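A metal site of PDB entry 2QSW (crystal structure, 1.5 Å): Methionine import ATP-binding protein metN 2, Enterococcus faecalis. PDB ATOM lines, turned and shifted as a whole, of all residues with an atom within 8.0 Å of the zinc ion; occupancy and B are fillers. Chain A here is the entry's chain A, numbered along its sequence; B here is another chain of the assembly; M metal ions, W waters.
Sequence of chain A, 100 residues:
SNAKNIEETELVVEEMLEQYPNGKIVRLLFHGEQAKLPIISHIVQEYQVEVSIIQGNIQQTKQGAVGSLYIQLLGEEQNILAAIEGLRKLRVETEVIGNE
The zinc ion is bound by ND1 of His 31 (1.9 Å), OE2 of Glu 33 (1.9 Å), OE1 of Glu 93 (2.0 Å) and water W1 (2.1 Å). Slightly farther from the zinc ion lies the side-chain carboxylate (OE1) of Glu 33 (2.8 Å). Slightly farther from the zinc ion lies the side-chain carboxylate (OE2) of Glu 93 (2.8 Å).
The side-chain amide oxygen (OE1) of Gln 34 lies within hydrogen-bond range of the backbone NH (N) of His 31, at 3.4 Å. O of Glu 33 sits close to NE of Arg 91, 3.4 Å away. The backbone carbonyl oxygen (O) of Glu 93 sits at hydrogen-bond distance from the backbone NH (N) of Leu 29 (2.9 Å).
Leu 29 touches the zinc ion (O to ZN, 3.9 Å). O of Arg 91 touches the zinc ion, at 3.7 Å. Of the 18 residues printed, 5 come within 4 Å of the zinc ion.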
ATOM      1  N   LEU A  28       0.617  35.768 -11.830  1.00  0.00           N
ATOM      2  CA  LEU A  28       1.003  34.916 -12.939  1.00  0.00           C
ATOM      3  C   LEU A  28       2.029  33.935 -12.380  1.00  0.00           C
ATOM      4  O   LEU A  28       2.991  34.368 -11.737  1.00  0.00           O
ATOM      5  CB  LEU A  28       1.677  35.736 -14.064  1.00  0.00           C
ATOM      6  CG  LEU A  28       0.809  36.543 -15.054  1.00  0.00           C
ATOM      7  CD1 LEU A  28      -0.019  37.658 -14.362  1.00  0.00           C
ATOM      8  CD2 LEU A  28       1.703  37.137 -16.142  1.00  0.00           C
ATOM      9  N   LEU A  29       1.860  32.646 -12.698  1.00  0.00           N
ATOM     10  CA  LEU A  29       2.836  31.594 -12.341  1.00  0.00           C
ATOM     11  C   LEU A  29       3.501  31.018 -13.575  1.00  0.00           C
ATOM     12  O   LEU A  29       2.826  30.796 -14.608  1.00  0.00           O
ATOM     13  CB  LEU A  29       2.132  30.444 -11.598  1.00  0.00           C
ATOM     14  CG  LEU A  29       1.426  30.821 -10.314  1.00  0.00           C
ATOM     15  CD1 LEU A  29       0.755  29.569  -9.623  1.00  0.00           C
ATOM     16  CD2 LEU A  29       2.345  31.614  -9.372  1.00  0.00           C
ATOM     17  N   PHE A  30       4.828  30.807 -13.483  1.00  0.00           N
ATOM     18  CA  PHE A  30       5.656  30.289 -14.579  1.00  0.00           C
ATOM     19  C   PHE A  30       6.317  29.043 -14.052  1.00  0.00           C
ATOM     20  O   PHE A  30       6.963  29.085 -13.014  1.00  0.00           O
ATOM     21  CB  PHE A  30       6.731  31.308 -14.978  1.00  0.00           C
ATOM     22  CG  PHE A  30       6.144  32.609 -15.481  1.00  0.00           C
ATOM     23  CD1 PHE A  30       5.787  32.766 -16.808  1.00  0.00           C
ATOM     24  CD2 PHE A  30       5.868  33.619 -14.599  1.00  0.00           C
ATOM     25  CE1 PHE A  30       5.218  33.953 -17.276  1.00  0.00           C
ATOM     26  CE2 PHE A  30       5.314  34.823 -15.068  1.00  0.00           C
ATOM     27  CZ  PHE A  30       4.987  34.976 -16.375  1.00  0.00           C
ATOM     28  N   HIS A  31       6.055  27.892 -14.696  1.00  0.00           N
ATOM     29  CA  HIS A  31       6.667  26.622 -14.289  1.00  0.00           C
ATOM     30  C   HIS A  31       7.610  26.089 -15.367  1.00  0.00           C
ATOM     31  O   HIS A  31       8.143  24.986 -15.231  1.00  0.00           O
ATOM     32  CB  HIS A  31       5.595  25.562 -14.021  1.00  0.00           C
ATOM     33  CG  HIS A  31       4.565  25.986 -13.022  1.00  0.00           C
ATOM     34  ND1 HIS A  31       3.344  26.595 -13.361  1.00  0.00           N
ATOM     35  CD2 HIS A  31       4.572  25.860 -11.671  1.00  0.00           C
ATOM     36  CE1 HIS A  31       2.669  26.821 -12.249  1.00  0.00           C
ATOM     37  NE2 HIS A  31       3.387  26.389 -11.213  1.00  0.00           N
ATOM     38  N   GLY A  32       7.833  26.846 -16.421  1.00  0.00           N
ATOM     39  CA  GLY A  32       8.680  26.463 -17.550  1.00  0.00           C
ATOM     40  C   GLY A  32       7.924  25.870 -18.703  1.00  0.00           C
ATOM     41  O   GLY A  32       8.518  25.629 -19.769  1.00  0.00           O
ATOM     42  N   GLU A  33       6.618  25.591 -18.498  1.00  0.00           N
ATOM     43  CA  GLU A  33       5.782  25.085 -19.556  1.00  0.00           C
ATOM     44  C   GLU A  33       5.080  26.172 -20.393  1.00  0.00           C
ATOM     45  O   GLU A  33       4.456  25.873 -21.415  1.00  0.00           O
ATOM     46  CB  GLU A  33       4.737  24.108 -18.995  1.00  0.00           C
ATOM     47  CG  GLU A  33       3.428  24.691 -18.484  1.00  0.00           C
ATOM     48  CD  GLU A  33       3.471  25.491 -17.171  1.00  0.00           C
ATOM     49  OE1 GLU A  33       4.539  26.038 -16.762  1.00  0.00           O
ATOM     50  OE2 GLU A  33       2.397  25.660 -16.524  1.00  0.00           O
ATOM     51  N   GLN A  34       5.203  27.418 -19.948  1.00  0.00           N
ATOM     52  CA  GLN A  34       4.547  28.525 -20.641  1.00  0.00           C
ATOM     53  C   GLN A  34       4.972  28.660 -22.102  1.00  0.00           C
ATOM     54  O   GLN A  34       6.072  28.258 -22.493  1.00  0.00           O
ATOM     55  CB  GLN A  34       4.791  29.846 -19.907  1.00  0.00           C
ATOM     56  CG  GLN A  34       6.273  30.239 -19.883  1.00  0.00           C
ATOM     57  CD  GLN A  34       7.018  29.761 -18.602  1.00  0.00           C
ATOM     58  OE1 GLN A  34       6.538  28.916 -17.857  1.00  0.00           O
ATOM     59  NE2 GLN A  34       8.227  30.329 -18.378  1.00  0.00           N
ATOM     60  N   ALA A  65      12.019  29.808 -17.488  1.00  0.00           N
ATOM     61  CA  ALA A  65      11.743  30.826 -16.481  1.00  0.00           C
ATOM     62  C   ALA A  65      10.705  30.284 -15.526  1.00  0.00           C
ATOM     63  O   ALA A  65       9.665  29.777 -15.967  1.00  0.00           O
ATOM     64  CB  ALA A  65      11.245  32.154 -17.067  1.00  0.00           C
ATOM     65  N   GLY A  67       8.691  30.931 -11.586  1.00  0.00           N
ATOM     66  CA  GLY A  67       8.377  31.808 -10.503  1.00  0.00           C
ATOM     67  C   GLY A  67       7.020  32.484 -10.619  1.00  0.00           C
ATOM     68  O   GLY A  67       6.118  31.916 -11.232  1.00  0.00           O
ATOM     69  N   ARG A  88      -3.768  32.298 -19.379  1.00  0.00           N
ATOM     70  CA  ARG A  88      -4.018  30.898 -19.001  1.00  0.00           C
ATOM     71  C   ARG A  88      -3.859  29.968 -20.186  1.00  0.00           C
ATOM     72  O   ARG A  88      -3.269  28.898 -20.077  1.00  0.00           O
ATOM     73  CB  ARG A  88      -5.415  30.755 -18.429  1.00  0.00           C
ATOM     74  CG  ARG A  88      -5.518  31.356 -17.036  1.00  0.00           C
ATOM     75  CD  ARG A  88      -6.948  31.515 -16.636  1.00  0.00           C
ATOM     76  NE  ARG A  88      -7.064  32.085 -15.298  1.00  0.00           N
ATOM     77  CZ  ARG A  88      -8.180  32.624 -14.823  1.00  0.00           C
ATOM     78  NH1 ARG A  88      -9.282  32.640 -15.573  1.00  0.00           N
ATOM     79  NH2 ARG A  88      -8.196  33.144 -13.610  1.00  0.00           N
ATOM     80  N   LEU A  90      -2.084  30.465 -22.836  1.00  0.00           N
ATOM     81  CA  LEU A  90      -0.641  30.466 -23.095  1.00  0.00           C
ATOM     82  C   LEU A  90       0.151  29.718 -22.001  1.00  0.00           C
ATOM     83  O   LEU A  90       1.387  29.748 -22.030  1.00  0.00           O
ATOM     84  CB  LEU A  90      -0.120  31.900 -23.245  1.00  0.00           C
ATOM     85  CG  LEU A  90      -0.711  32.649 -24.466  1.00  0.00           C
ATOM     86  CD1 LEU A  90      -0.243  34.122 -24.388  1.00  0.00           C
ATOM     87  CD2 LEU A  90      -0.318  31.959 -25.796  1.00  0.00           C
ATOM     88  N   ARG A  91      -0.528  29.015 -21.088  1.00  0.00           N
ATOM     89  CA  ARG A  91       0.077  28.129 -20.071  1.00  0.00           C
ATOM     90  C   ARG A  91       0.790  28.912 -18.991  1.00  0.00           C
ATOM     91  O   ARG A  91       1.772  28.470 -18.388  1.00  0.00           O
ATOM     92  CB  ARG A  91       0.908  27.023 -20.737  1.00  0.00           C
ATOM     93  CG  ARG A  91       0.112  26.243 -21.821  1.00  0.00           C
ATOM     94  CD  ARG A  91       0.923  25.378 -22.791  1.00  0.00           C
ATOM     95  NE  ARG A  91       1.550  24.279 -22.067  1.00  0.00           N
ATOM     96  CZ  ARG A  91       2.475  23.448 -22.568  1.00  0.00           C
ATOM     97  NH1 ARG A  91       2.941  23.602 -23.785  1.00  0.00           N
ATOM     98  NH2 ARG A  91       2.983  22.502 -21.773  1.00  0.00           N
ATOM     99  N   VAL A  92       0.247  30.107 -18.713  1.00  0.00           N
ATOM    100  CA  VAL A  92       0.612  30.889 -17.575  1.00  0.00           C
ATOM    101  C   VAL A  92      -0.611  30.929 -16.631  1.00  0.00           C
ATOM    102  O   VAL A  92      -1.579  31.666 -16.883  1.00  0.00           O
ATOM    103  CB  VAL A  92       1.030  32.372 -17.990  1.00  0.00           C
ATOM    104  CG1 VAL A  92       1.317  33.172 -16.742  1.00  0.00           C
ATOM    105  CG2 VAL A  92       2.193  32.391 -18.961  1.00  0.00           C
ATOM    106  N   GLU A  93      -0.543  30.179 -15.553  1.00  0.00           N
ATOM    107  CA  GLU A  93      -1.644  30.157 -14.567  1.00  0.00           C
ATOM    108  C   GLU A  93      -1.798  31.556 -13.969  1.00  0.00           C
ATOM    109  O   GLU A  93      -0.829  32.176 -13.548  1.00  0.00           O
ATOM    110  CB  GLU A  93      -1.400  29.159 -13.476  1.00  0.00           C
ATOM    111  CG  GLU A  93      -1.438  27.714 -13.911  1.00  0.00           C
ATOM    112  CD  GLU A  93      -0.071  27.115 -14.252  1.00  0.00           C
ATOM    113  OE1 GLU A  93       0.852  27.897 -14.609  1.00  0.00           O
ATOM    114  OE2 GLU A  93       0.088  25.894 -14.135  1.00  0.00           O
ATOM    115  N   THR A  94      -3.020  32.073 -13.960  1.00  0.00           N
ATOM    116  CA  THR A  94      -3.261  33.465 -13.626  1.00  0.00           C
ATOM    117  C   THR A  94      -4.517  33.535 -12.785  1.00  0.00           C
ATOM    118  O   THR A  94      -5.523  32.902 -13.083  1.00  0.00           O
ATOM    119  CB  THR A  94      -3.423  34.282 -14.916  1.00  0.00           C
ATOM    120  OG1 THR A  94      -2.259  34.138 -15.757  1.00  0.00           O
ATOM    121  CG2 THR A  94      -3.612  35.772 -14.599  1.00  0.00           C
ATOM    122  N   GLY B  98      -7.457  25.790 -10.168  1.00  0.00           N
ATOM    123  CA  GLY B  98      -6.342  25.291 -11.002  1.00  0.00           C
ATOM    124  C   GLY B  98      -5.305  26.313 -11.404  1.00  0.00           C
ATOM    125  O   GLY B  98      -4.469  26.046 -12.315  1.00  0.00           O
ATOM    126  N   ASN B  99      -5.366  27.470 -10.760  1.00  0.00           N
ATOM    127  CA  ASN B  99      -4.381  28.536 -11.041  1.00  0.00           C
ATOM    128  C   ASN B  99      -3.442  28.833  -9.890  1.00  0.00           C
ATOM    129  O   ASN B  99      -2.779  29.888  -9.888  1.00  0.00           O
ATOM    130  CB  ASN B  99      -5.090  29.803 -11.546  1.00  0.00           C
ATOM    131  CG  ASN B  99      -5.652  29.601 -12.934  1.00  0.00           C
ATOM    132  OD1 ASN B  99      -4.938  29.633 -13.935  1.00  0.00           O
ATOM    133  ND2 ASN B  99      -6.949  29.299 -13.000  1.00  0.00           N
ATOM    134  N   GLU B 100      -3.314  27.879  -8.963  1.00  0.00           N
ATOM    135  CA  GLU B 100      -2.341  27.998  -7.900  1.00  0.00           C
ATOM    136  C   GLU B 100      -1.195  27.037  -8.283  1.00  0.00           C
ATOM    137  O   GLU B 100      -0.124  27.066  -7.678  1.00  0.00           O
ATOM    138  CB  GLU B 100      -2.922  27.659  -6.514  1.00  0.00           C
ATOM    139  CG  GLU B 100      -4.440  27.892  -6.217  1.00  0.00           C
ATOM    140  CD  GLU B 100      -4.827  29.239  -5.523  1.00  0.00           C
ATOM    141  OE1 GLU B 100      -6.020  29.489  -5.300  1.00  0.00           O
ATOM    142  OE2 GLU B 100      -3.980  30.068  -5.185  1.00  0.00           O
ATOM    143  OXT GLU B 100      -1.267  26.194  -9.224  1.00  0.00           O
HETATM  144 ZN    ZN M   1       2.519  26.942 -15.076  1.00  0.00          ZN
HETATM  145  O   HOH W   1       3.243  28.634 -16.125  1.00  0.00           O
